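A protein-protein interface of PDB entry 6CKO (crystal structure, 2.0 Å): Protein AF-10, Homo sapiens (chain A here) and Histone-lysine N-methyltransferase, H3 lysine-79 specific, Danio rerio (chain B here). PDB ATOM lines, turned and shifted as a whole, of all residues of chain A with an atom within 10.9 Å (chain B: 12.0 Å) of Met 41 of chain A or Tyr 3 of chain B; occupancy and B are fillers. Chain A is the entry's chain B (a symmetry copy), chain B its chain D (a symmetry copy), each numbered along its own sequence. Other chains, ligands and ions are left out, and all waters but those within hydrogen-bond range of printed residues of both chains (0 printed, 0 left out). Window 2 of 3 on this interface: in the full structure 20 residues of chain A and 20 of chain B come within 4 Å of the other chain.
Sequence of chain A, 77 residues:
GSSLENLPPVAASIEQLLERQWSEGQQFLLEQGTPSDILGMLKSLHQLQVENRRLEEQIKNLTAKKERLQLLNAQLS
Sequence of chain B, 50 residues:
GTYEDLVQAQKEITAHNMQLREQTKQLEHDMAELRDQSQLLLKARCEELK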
ATOM      1  N   TRP A  22      12.860  17.204 -14.145  1.00  0.00           N
ATOM      2  CA  TRP A  22      12.401  15.824 -14.076  1.00  0.00           C
ATOM      3  C   TRP A  22      13.526  14.785 -14.342  1.00  0.00           C
ATOM      4  O   TRP A  22      13.614  13.790 -13.612  1.00  0.00           O
ATOM      5  CB  TRP A  22      11.250  15.591 -15.053  1.00  0.00           C
ATOM      6  CG  TRP A  22      11.067  14.167 -15.459  1.00  0.00           C
ATOM      7  CD1 TRP A  22      11.419  13.597 -16.657  1.00  0.00           C
ATOM      8  CD2 TRP A  22      10.504  13.132 -14.671  1.00  0.00           C
ATOM      9  NE1 TRP A  22      11.105  12.258 -16.655  1.00  0.00           N
ATOM     10  CE2 TRP A  22      10.536  11.946 -15.448  1.00  0.00           C
ATOM     11  CE3 TRP A  22       9.976  13.081 -13.369  1.00  0.00           C
ATOM     12  CZ2 TRP A  22      10.040  10.726 -14.976  1.00  0.00           C
ATOM     13  CZ3 TRP A  22       9.481  11.866 -12.899  1.00  0.00           C
ATOM     14  CH2 TRP A  22       9.524  10.705 -13.701  1.00  0.00           C
ATOM     15  N   GLN A  26      14.621  11.912 -11.737  1.00  0.00           N
ATOM     16  CA  GLN A  26      14.663  10.500 -12.103  1.00  0.00           C
ATOM     17  C   GLN A  26      16.089   9.961 -11.930  1.00  0.00           C
ATOM     18  O   GLN A  26      16.256   8.911 -11.349  1.00  0.00           O
ATOM     19  CB  GLN A  26      14.170  10.253 -13.542  1.00  0.00           C
ATOM     20  CG  GLN A  26      13.351   8.973 -13.707  1.00  0.00           C
ATOM     21  N   LEU A  29      16.630   9.512  -8.084  1.00  0.00           N
ATOM     22  CA  LEU A  29      15.869   8.409  -7.470  1.00  0.00           C
ATOM     23  C   LEU A  29      16.427   7.019  -7.868  1.00  0.00           C
ATOM     24  O   LEU A  29      16.535   6.113  -7.035  1.00  0.00           O
ATOM     25  CB  LEU A  29      14.393   8.520  -7.857  1.00  0.00           C
ATOM     26  CG  LEU A  29      13.672   9.733  -7.252  1.00  0.00           C
ATOM     27  CD1 LEU A  29      12.266   9.794  -7.812  1.00  0.00           C
ATOM     28  CD2 LEU A  29      13.665   9.678  -5.737  1.00  0.00           C
ATOM     29  N   THR A  34      15.249   3.479  -6.024  1.00  0.00           N
ATOM     30  CA  THR A  34      13.807   3.453  -5.803  1.00  0.00           C
ATOM     31  C   THR A  34      13.166   2.308  -6.611  1.00  0.00           C
ATOM     32  O   THR A  34      13.488   2.144  -7.771  1.00  0.00           O
ATOM     33  CB  THR A  34      13.222   4.786  -6.326  1.00  0.00           C
ATOM     34  OG1 THR A  34      14.018   5.876  -5.845  1.00  0.00           O
ATOM     35  CG2 THR A  34      11.793   4.974  -5.909  1.00  0.00           C
ATOM     36  N   PRO A  35      12.210   1.557  -6.034  1.00  0.00           N
ATOM     37  CA  PRO A  35      11.583   0.460  -6.801  1.00  0.00           C
ATOM     38  C   PRO A  35      10.996   0.804  -8.178  1.00  0.00           C
ATOM     39  O   PRO A  35      10.396   1.884  -8.365  1.00  0.00           O
ATOM     40  CB  PRO A  35      10.448  -0.026  -5.881  1.00  0.00           C
ATOM     41  CG  PRO A  35      10.765   0.489  -4.527  1.00  0.00           C
ATOM     42  CD  PRO A  35      11.878   1.492  -4.599  1.00  0.00           C
ATOM     43  N   SER A  36      11.082  -0.154  -9.101  1.00  0.00           N
ATOM     44  CA  SER A  36      10.622   0.022 -10.484  1.00  0.00           C
ATOM     45  C   SER A  36       9.176   0.524 -10.579  1.00  0.00           C
ATOM     46  O   SER A  36       8.848   1.339 -11.456  1.00  0.00           O
ATOM     47  CB  SER A  36      10.747  -1.286 -11.274  1.00  0.00           C
ATOM     48  N   ASP A  37       8.324   0.030  -9.684  1.00  0.00           N
ATOM     49  CA  ASP A  37       6.905   0.380  -9.702  1.00  0.00           C
ATOM     50  C   ASP A  37       6.659   1.840  -9.328  1.00  0.00           C
ATOM     51  O   ASP A  37       5.924   2.533 -10.005  1.00  0.00           O
ATOM     52  CB  ASP A  37       6.123  -0.572  -8.787  1.00  0.00           C
ATOM     53  CG  ASP A  37       5.974  -1.957  -9.387  1.00  0.00           C
ATOM     54  OD1 ASP A  37       5.802  -2.063 -10.617  1.00  0.00           O
ATOM     55  OD2 ASP A  37       6.011  -2.945  -8.631  1.00  0.00           O
ATOM     56  N   ILE A  38       7.291   2.287  -8.249  1.00  0.00           N
ATOM     57  CA  ILE A  38       7.263   3.675  -7.825  1.00  0.00           C
ATOM     58  C   ILE A  38       7.799   4.597  -8.918  1.00  0.00           C
ATOM     59  O   ILE A  38       7.170   5.627  -9.211  1.00  0.00           O
ATOM     60  CB  ILE A  38       8.008   3.871  -6.492  1.00  0.00           C
ATOM     61  CG1 ILE A  38       7.201   3.243  -5.343  1.00  0.00           C
ATOM     62  CG2 ILE A  38       8.263   5.336  -6.162  1.00  0.00           C
ATOM     63  N   LEU A  39       8.922   4.226  -9.544  1.00  0.00           N
ATOM     64  CA  LEU A  39       9.451   5.006 -10.665  1.00  0.00           C
ATOM     65  C   LEU A  39       8.503   5.048 -11.842  1.00  0.00           C
ATOM     66  O   LEU A  39       8.373   6.083 -12.490  1.00  0.00           O
ATOM     67  CB  LEU A  39      10.773   4.437 -11.188  1.00  0.00           C
ATOM     68  CG  LEU A  39      11.941   4.535 -10.212  1.00  0.00           C
ATOM     69  CD1 LEU A  39      13.150   3.772 -10.743  1.00  0.00           C
ATOM     70  CD2 LEU A  39      12.260   6.014  -9.961  1.00  0.00           C
ATOM     71  N   GLY A  40       7.909   3.907 -12.158  1.00  0.00           N
ATOM     72  CA  GLY A  40       6.957   3.818 -13.245  1.00  0.00           C
ATOM     73  C   GLY A  40       5.691   4.620 -12.978  1.00  0.00           C
ATOM     74  O   GLY A  40       5.092   5.135 -13.908  1.00  0.00           O
ATOM     75  N   MET A  41       5.305   4.708 -11.704  1.00  0.00           N
ATOM     76  CA  MET A  41       4.206   5.555 -11.266  1.00  0.00           C
ATOM     77  C   MET A  41       4.561   7.013 -11.434  1.00  0.00           C
ATOM     78  O   MET A  41       3.806   7.748 -12.094  1.00  0.00           O
ATOM     79  CB  MET A  41       3.860   5.267  -9.812  1.00  0.00           C
ATOM     80  CG  MET A  41       2.639   5.978  -9.270  1.00  0.00           C
ATOM     81  SD  MET A  41       1.746   4.937  -8.080  1.00  0.00           S
ATOM     82  CE  MET A  41       3.048   4.241  -7.048  1.00  0.00           C
ATOM     83  N   LEU A  42       5.695   7.433 -10.867  1.00  0.00           N
ATOM     84  CA  LEU A  42       6.160   8.820 -11.019  1.00  0.00           C
ATOM     85  C   LEU A  42       6.298   9.276 -12.484  1.00  0.00           C
ATOM     86  O   LEU A  42       6.018  10.451 -12.779  1.00  0.00           O
ATOM     87  CB  LEU A  42       7.496   9.084 -10.314  1.00  0.00           C
ATOM     88  CG  LEU A  42       7.502   9.175  -8.787  1.00  0.00           C
ATOM     89  CD1 LEU A  42       8.834   8.682  -8.237  1.00  0.00           C
ATOM     90  CD2 LEU A  42       7.196  10.578  -8.261  1.00  0.00           C
ATOM     91  N   LYS A  43       6.712   8.368 -13.381  1.00  0.00           N
ATOM     92  CA  LYS A  43       6.931   8.734 -14.776  1.00  0.00           C
ATOM     93  C   LYS A  43       5.618   9.024 -15.512  1.00  0.00           C
ATOM     94  O   LYS A  43       5.538   9.984 -16.252  1.00  0.00           O
ATOM     95  CB  LYS A  43       7.742   7.666 -15.519  1.00  0.00           C
ATOM     96  CG  LYS A  43       8.261   8.135 -16.874  1.00  0.00           C
ATOM     97  N   SER A  44       4.610   8.180 -15.301  1.00  0.00           N
ATOM     98  CA  SER A  44       3.289   8.381 -15.883  1.00  0.00           C
ATOM     99  C   SER A  44       2.644   9.631 -15.300  1.00  0.00           C
ATOM    100  O   SER A  44       1.974  10.368 -16.027  1.00  0.00           O
ATOM    101  CB  SER A  44       2.399   7.171 -15.632  1.00  0.00           C
ATOM    102  OG  SER A  44       2.474   6.803 -14.277  1.00  0.00           O
ATOM    103  N   LEU A  45       2.866   9.895 -14.009  1.00  0.00           N
ATOM    104  CA  LEU A  45       2.452  11.174 -13.434  1.00  0.00           C
ATOM    105  C   LEU A  45       3.069  12.352 -14.161  1.00  0.00           C
ATOM    106  O   LEU A  45       2.334  13.262 -14.615  1.00  0.00           O
ATOM    107  CB  LEU A  45       2.747  11.287 -11.945  1.00  0.00           C
ATOM    108  CG  LEU A  45       2.019  10.280 -11.030  1.00  0.00           C
ATOM    109  CD1 LEU A  45       2.036  10.752  -9.578  1.00  0.00           C
ATOM    110  CD2 LEU A  45       0.600   9.963 -11.475  1.00  0.00           C
ATOM    111  N   HIS A  46       4.399  12.340 -14.255  1.00  0.00           N
ATOM    112  CA  HIS A  46       5.138  13.354 -15.012  1.00  0.00           C
ATOM    113  C   HIS A  46       4.523  13.578 -16.398  1.00  0.00           C
ATOM    114  O   HIS A  46       4.290  14.709 -16.776  1.00  0.00           O
ATOM    115  CB  HIS A  46       6.611  12.972 -15.146  1.00  0.00           C
ATOM    116  CG  HIS A  46       7.311  13.646 -16.274  1.00  0.00           C
ATOM    117  ND1 HIS A  46       7.692  14.966 -16.226  1.00  0.00           N
ATOM    118  CD2 HIS A  46       7.681  13.187 -17.490  1.00  0.00           C
ATOM    119  CE1 HIS A  46       8.277  15.293 -17.360  1.00  0.00           C
ATOM    120  NE2 HIS A  46       8.281  14.230 -18.146  1.00  0.00           N
ATOM    121  N   GLN A  47       4.289  12.497 -17.141  1.00  0.00           N
ATOM    122  CA  GLN A  47       3.782  12.596 -18.506  1.00  0.00           C
ATOM    123  C   GLN A  47       2.355  13.177 -18.526  1.00  0.00           C
ATOM    124  O   GLN A  47       2.043  14.029 -19.358  1.00  0.00           O
ATOM    125  CB  GLN A  47       3.885  11.255 -19.231  1.00  0.00           C
ATOM    126  CG  GLN A  47       5.356  10.897 -19.469  1.00  0.00           C
ATOM    127  CD  GLN A  47       5.571   9.665 -20.314  1.00  0.00           C
ATOM    128  OE1 GLN A  47       4.990   8.612 -20.061  1.00  0.00           O
ATOM    129  NE2 GLN A  47       6.443   9.784 -21.318  1.00  0.00           N
ATOM    130  N   LEU A  48       1.514  12.761 -17.591  1.00  0.00           N
ATOM    131  CA  LEU A  48       0.193  13.386 -17.469  1.00  0.00           C
ATOM    132  C   LEU A  48       0.287  14.893 -17.152  1.00  0.00           C
ATOM    133  O   LEU A  48      -0.454  15.707 -17.742  1.00  0.00           O
ATOM    134  CB  LEU A  48      -0.680  12.641 -16.455  1.00  0.00           C
ATOM    135  CG  LEU A  48      -1.251  11.319 -16.948  1.00  0.00           C
ATOM    136  CD1 LEU A  48      -1.748  10.505 -15.779  1.00  0.00           C
ATOM    137  CD2 LEU A  48      -2.378  11.463 -17.957  1.00  0.00           C
ATOM    138  N   GLN A  49       1.177  15.282 -16.242  1.00  0.00           N
ATOM    139  CA  GLN A  49       1.406  16.710 -15.976  1.00  0.00           C
ATOM    140  C   GLN A  49       1.877  17.501 -17.214  1.00  0.00           C
ATOM    141  O   GLN A  49       1.454  18.617 -17.398  1.00  0.00           O
ATOM    142  CB  GLN A  49       2.374  16.939 -14.823  1.00  0.00           C
ATOM    143  CG  GLN A  49       1.757  16.626 -13.467  1.00  0.00           C
ATOM    144  CD  GLN A  49       2.779  16.545 -12.360  1.00  0.00           C
ATOM    145  OE1 GLN A  49       3.858  15.941 -12.517  1.00  0.00           O
ATOM    146  NE2 GLN A  49       2.467  17.160 -11.238  1.00  0.00           N
ATOM    147  N   GLY B   1       1.012   7.008   3.733  1.00  0.00           N
ATOM    148  CA  GLY B   1       2.381   7.522   3.509  1.00  0.00           C
ATOM    149  C   GLY B   1       2.519   7.959   2.068  1.00  0.00           C
ATOM    150  O   GLY B   1       1.506   8.228   1.386  1.00  0.00           O
ATOM    151  N   THR B   2       3.766   7.989   1.599  1.00  0.00           N
ATOM    152  CA  THR B   2       4.067   8.500   0.270  1.00  0.00           C
ATOM    153  C   THR B   2       3.481   7.592  -0.832  1.00  0.00           C
ATOM    154  O   THR B   2       3.013   8.094  -1.868  1.00  0.00           O
ATOM    155  CB  THR B   2       5.564   8.834   0.103  1.00  0.00           C
ATOM    156  OG1 THR B   2       6.348   7.716   0.487  1.00  0.00           O
ATOM    157  CG2 THR B   2       5.984  10.063   1.020  1.00  0.00           C
ATOM    158  N   TYR B   3       3.383   6.291  -0.584  1.00  0.00           N
ATOM    159  CA  TYR B   3       2.721   5.433  -1.560  1.00  0.00           C
ATOM    160  C   TYR B   3       1.234   5.825  -1.767  1.00  0.00           C
ATOM    161  O   TYR B   3       0.789   5.967  -2.903  1.00  0.00           O
ATOM    162  CB  TYR B   3       2.859   3.942  -1.260  1.00  0.00           C
ATOM    163  CG  TYR B   3       2.117   3.126  -2.276  1.00  0.00           C
ATOM    164  CD1 TYR B   3       2.625   2.967  -3.564  1.00  0.00           C
ATOM    165  CD2 TYR B   3       0.870   2.577  -1.985  1.00  0.00           C
ATOM    166  CE1 TYR B   3       1.925   2.247  -4.528  1.00  0.00           C
ATOM    167  CE2 TYR B   3       0.164   1.843  -2.935  1.00  0.00           C
ATOM    168  CZ  TYR B   3       0.693   1.679  -4.211  1.00  0.00           C
ATOM    169  OH  TYR B   3      -0.006   0.976  -5.190  1.00  0.00           O
ATOM    170  N   GLU B   4       0.496   5.993  -0.674  1.00  0.00           N
ATOM    171  CA  GLU B   4      -0.910   6.353  -0.717  1.00  0.00           C
ATOM    172  C   GLU B   4      -1.085   7.773  -1.291  1.00  0.00           C
ATOM    173  O   GLU B   4      -2.055   8.030  -1.997  1.00  0.00           O
ATOM    174  CB  GLU B   4      -1.547   6.282   0.674  1.00  0.00           C
ATOM    175  CG  GLU B   4      -1.713   4.879   1.245  1.00  0.00           C
ATOM    176  CD  GLU B   4      -0.426   4.208   1.746  1.00  0.00           C
ATOM    177  OE1 GLU B   4       0.519   4.885   2.232  1.00  0.00           O
ATOM    178  OE2 GLU B   4      -0.363   2.955   1.640  1.00  0.00           O
ATOM    179  N   ASP B   5      -0.143   8.675  -0.965  1.00  0.00           N
ATOM    180  CA  ASP B   5      -0.071   9.993  -1.546  1.00  0.00           C
ATOM    181  C   ASP B   5       0.082   9.959  -3.090  1.00  0.00           C
ATOM    182  O   ASP B   5      -0.598  10.728  -3.805  1.00  0.00           O
ATOM    183  CB  ASP B   5       1.014  10.844  -0.871  1.00  0.00           C
ATOM    184  CG  ASP B   5       0.664  11.233   0.586  1.00  0.00           C
ATOM    185  OD1 ASP B   5      -0.492  11.105   0.984  1.00  0.00           O
ATOM    186  OD2 ASP B   5       1.522  11.680   1.358  1.00  0.00           O
ATOM    187  N   LEU B   6       0.945   9.073  -3.601  1.00  0.00           N
ATOM    188  CA  LEU B   6       1.124   8.909  -5.051  1.00  0.00           C
ATOM    189  C   LEU B   6      -0.102   8.348  -5.756  1.00  0.00           C
ATOM    190  O   LEU B   6      -0.455   8.824  -6.832  1.00  0.00           O
ATOM    191  CB  LEU B   6       2.359   8.067  -5.382  1.00  0.00           C
ATOM    192  CG  LEU B   6       3.694   8.768  -5.086  1.00  0.00           C
ATOM    193  CD1 LEU B   6       4.870   7.853  -5.359  1.00  0.00           C
ATOM    194  CD2 LEU B   6       3.813  10.050  -5.906  1.00  0.00           C
ATOM    195  N   VAL B   7      -0.754   7.367  -5.140  1.00  0.00           N
ATOM    196  CA  VAL B   7      -2.039   6.905  -5.602  1.00  0.00           C
ATOM    197  C   VAL B   7      -3.051   8.049  -5.640  1.00  0.00           C
ATOM    198  O   VAL B   7      -3.759   8.198  -6.656  1.00  0.00           O
ATOM    199  CB  VAL B   7      -2.618   5.720  -4.774  1.00  0.00           C
ATOM    200  CG1 VAL B   7      -4.077   5.447  -5.151  1.00  0.00           C
ATOM    201  CG2 VAL B   7      -1.794   4.466  -5.019  1.00  0.00           C
ATOM    202  N   GLN B   8      -3.128   8.853  -4.576  1.00  0.00           N
ATOM    203  CA  GLN B   8      -4.063   9.959  -4.562  1.00  0.00           C
ATOM    204  C   GLN B   8      -3.697  10.997  -5.652  1.00  0.00           C
ATOM    205  O   GLN B   8      -4.605  11.485  -6.397  1.00  0.00           O
ATOM    206  CB  GLN B   8      -4.197  10.585  -3.169  1.00  0.00           C
ATOM    207  CG  GLN B   8      -5.150  11.795  -3.050  1.00  0.00           C
ATOM    208  CD  GLN B   8      -6.602  11.512  -3.438  1.00  0.00           C
ATOM    209  OE1 GLN B   8      -7.105  10.417  -3.213  1.00  0.00           O
ATOM    210  NE2 GLN B   8      -7.286  12.514  -4.023  1.00  0.00           N
ATOM    211  N   ALA B   9      -2.415  11.356  -5.748  1.00  0.00           N
ATOM    212  CA  ALA B   9      -2.003  12.288  -6.783  1.00  0.00           C
ATOM    213  C   ALA B   9      -2.402  11.785  -8.203  1.00  0.00           C
ATOM    214  O   ALA B   9      -2.890  12.558  -9.049  1.00  0.00           O
ATOM    215  CB  ALA B   9      -0.514  12.546  -6.723  1.00  0.00           C
ATOM    216  N   GLN B  10      -2.155  10.508  -8.453  1.00  0.00           N
ATOM    217  CA  GLN B  10      -2.524   9.878  -9.718  1.00  0.00           C
ATOM    218  C   GLN B  10      -3.988  10.035 -10.041  1.00  0.00           C
ATOM    219  O   GLN B  10      -4.328  10.416 -11.141  1.00  0.00           O
ATOM    220  CB  GLN B  10      -2.237   8.408  -9.686  1.00  0.00           C
ATOM    221  CG  GLN B  10      -2.493   7.673 -10.976  1.00  0.00           C
ATOM    222  CD  GLN B  10      -1.899   6.307 -10.864  1.00  0.00           C
ATOM    223  OE1 GLN B  10      -2.300   5.534  -9.983  1.00  0.00           O
ATOM    224  NE2 GLN B  10      -0.881   6.024 -11.678  1.00  0.00           N
ATOM    225  N   LYS B  11      -4.827   9.711  -9.078  1.00  0.00           N
ATOM    226  CA  LYS B  11      -6.251   9.904  -9.203  1.00  0.00           C
ATOM    227  C   LYS B  11      -6.602  11.350  -9.608  1.00  0.00           C
ATOM    228  O   LYS B  11      -7.359  11.538 -10.534  1.00  0.00           O
ATOM    229  CB  LYS B  11      -6.923   9.514  -7.883  1.00  0.00           C
ATOM    230  CG  LYS B  11      -8.427   9.670  -7.787  1.00  0.00           C
ATOM    231  CD  LYS B  11      -8.901   9.092  -6.445  1.00  0.00           C
ATOM    232  CE  LYS B  11     -10.372   9.367  -6.185  1.00  0.00           C
ATOM    233  NZ  LYS B  11     -10.642  10.833  -6.152  1.00  0.00           N
ATOM    234  N   GLU B  12      -6.072  12.344  -8.882  1.00  0.00           N
ATOM    235  CA  GLU B  12      -6.395  13.741  -9.134  1.00  0.00           C
ATOM    236  C   GLU B  12      -5.857  14.226 -10.502  1.00  0.00           C
ATOM    237  O   GLU B  12      -6.567  14.876 -11.252  1.00  0.00           O
ATOM    238  CB  GLU B  12      -5.839  14.634  -8.035  1.00  0.00           C
ATOM    239  CG  GLU B  12      -6.529  14.420  -6.704  1.00  0.00           C
ATOM    240  CD  GLU B  12      -5.901  15.249  -5.592  1.00  0.00           C
ATOM    241  OE1 GLU B  12      -5.300  16.303  -5.919  1.00  0.00           O
ATOM    242  OE2 GLU B  12      -6.021  14.859  -4.412  1.00  0.00           O
ATOM    243  N   ILE B  13      -4.629  13.857 -10.824  1.00  0.00           N
ATOM    244  CA  ILE B  13      -4.002  14.278 -12.083  1.00  0.00           C
ATOM    245  C   ILE B  13      -4.739  13.652 -13.275  1.00  0.00           C
ATOM    246  O   ILE B  13      -4.958  14.320 -14.277  1.00  0.00           O
ATOM    247  CB  ILE B  13      -2.491  13.970 -12.068  1.00  0.00           C
ATOM    248  CG1 ILE B  13      -1.824  14.898 -11.049  1.00  0.00           C
ATOM    249  CG2 ILE B  13      -1.848  14.149 -13.436  1.00  0.00           C
ATOM    250  CD1 ILE B  13      -0.419  14.502 -10.665  1.00  0.00           C
ATOM    251  N   THR B  14      -5.146  12.393 -13.122  1.00  0.00           N
ATOM    252  CA  THR B  14      -5.894  11.678 -14.138  1.00  0.00           C
ATOM    253  C   THR B  14      -7.312  12.261 -14.332  1.00  0.00           C
ATOM    254  O   THR B  14      -7.762  12.418 -15.469  1.00  0.00           O
ATOM    255  CB  THR B  14      -5.954  10.174 -13.825  1.00  0.00           C
ATOM    256  OG1 THR B  14      -4.616   9.664 -13.670  1.00  0.00           O
ATOM    257  CG2 THR B  14      -6.693   9.400 -14.979  1.00  0.00           C
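O of Met 41 of chain A lies within hydrogen-bond range of OG of Ser 44 of chain A (2.7 Å). The side-chain hydroxyl (OG1) of Thr 14 of chain B lies within hydrogen-bond range of the backbone carbonyl oxygen (O) of Gln 10 of chain B (2.7 Å).
Tyr 3 of chain B touches Met 41 of chain A (CE1 to CE, 3.4 Å). Leu 45 of chain A touches Gln 10 of chain B. CB of Leu 48 of chain A touches CG2 of Ile 13 of chain B (3.6 Å). Thr 14 of chain B touches Leu 48 of chain A (OG1 to CD1, 3.7 Å). CD1 of Ile 13 of chain B touches NE2 of Gln 49 of chain A (3.97 Å).
No residue of chain B comes within 4 Å of Gly 40 of chain A. Of chain B, only Tyr 3 (3.4 Å) comes within 4 Å of Met 41 of chain A. No residue of chain B comes within 4 Å of Leu 42 of chain A. No residue of chain B comes within 4 Å of Ser 44 of chain A. Printed residues of chain B within 4 Å of Leu 48 of chain A: Ile 13 and Thr 14. Of the printed residues of chain B, Gln 49 of chain A touches Ile 13. No residue of chain A comes within 4 Å of Thr 2 of chain B. Tyr 3 of chain B touches one residue of chain A. No residue of chain A comes within 4 Å of Glu 4 of chain B. No residue of chain A comes within 4 Å of Asp 5 of chain B. Printed residues of chain A within 4 Å of Gln 10 of chain B: Leu 45. Of the printed residues of chain A, Ile 13 of chain B touches Leu 48 and Gln 49. The nearest printed residue of chain B that does not touch Leu 48 of chain A is Gln 10 of chain B (5.3 Å).
Hydrophobic or aromatic side chains of chain B within 4 Å of the printed part of chain A: Tyr 3 and Ile 13. Along chain B the printed residues that touch a printed residue of chain A span positions 3 to 14. Of the 19 printed residues of chain A, 4 touch a printed residue of chain B. Hydrophobic or aromatic side chains of chain A within 4 Å of the printed part of chain B: Met 41, Leu 45 and Leu 48. Among the printed residues, no Asp or Glu carboxylate lies within 4 Å of a Lys or Arg side-chain nitrogen of the other chain.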
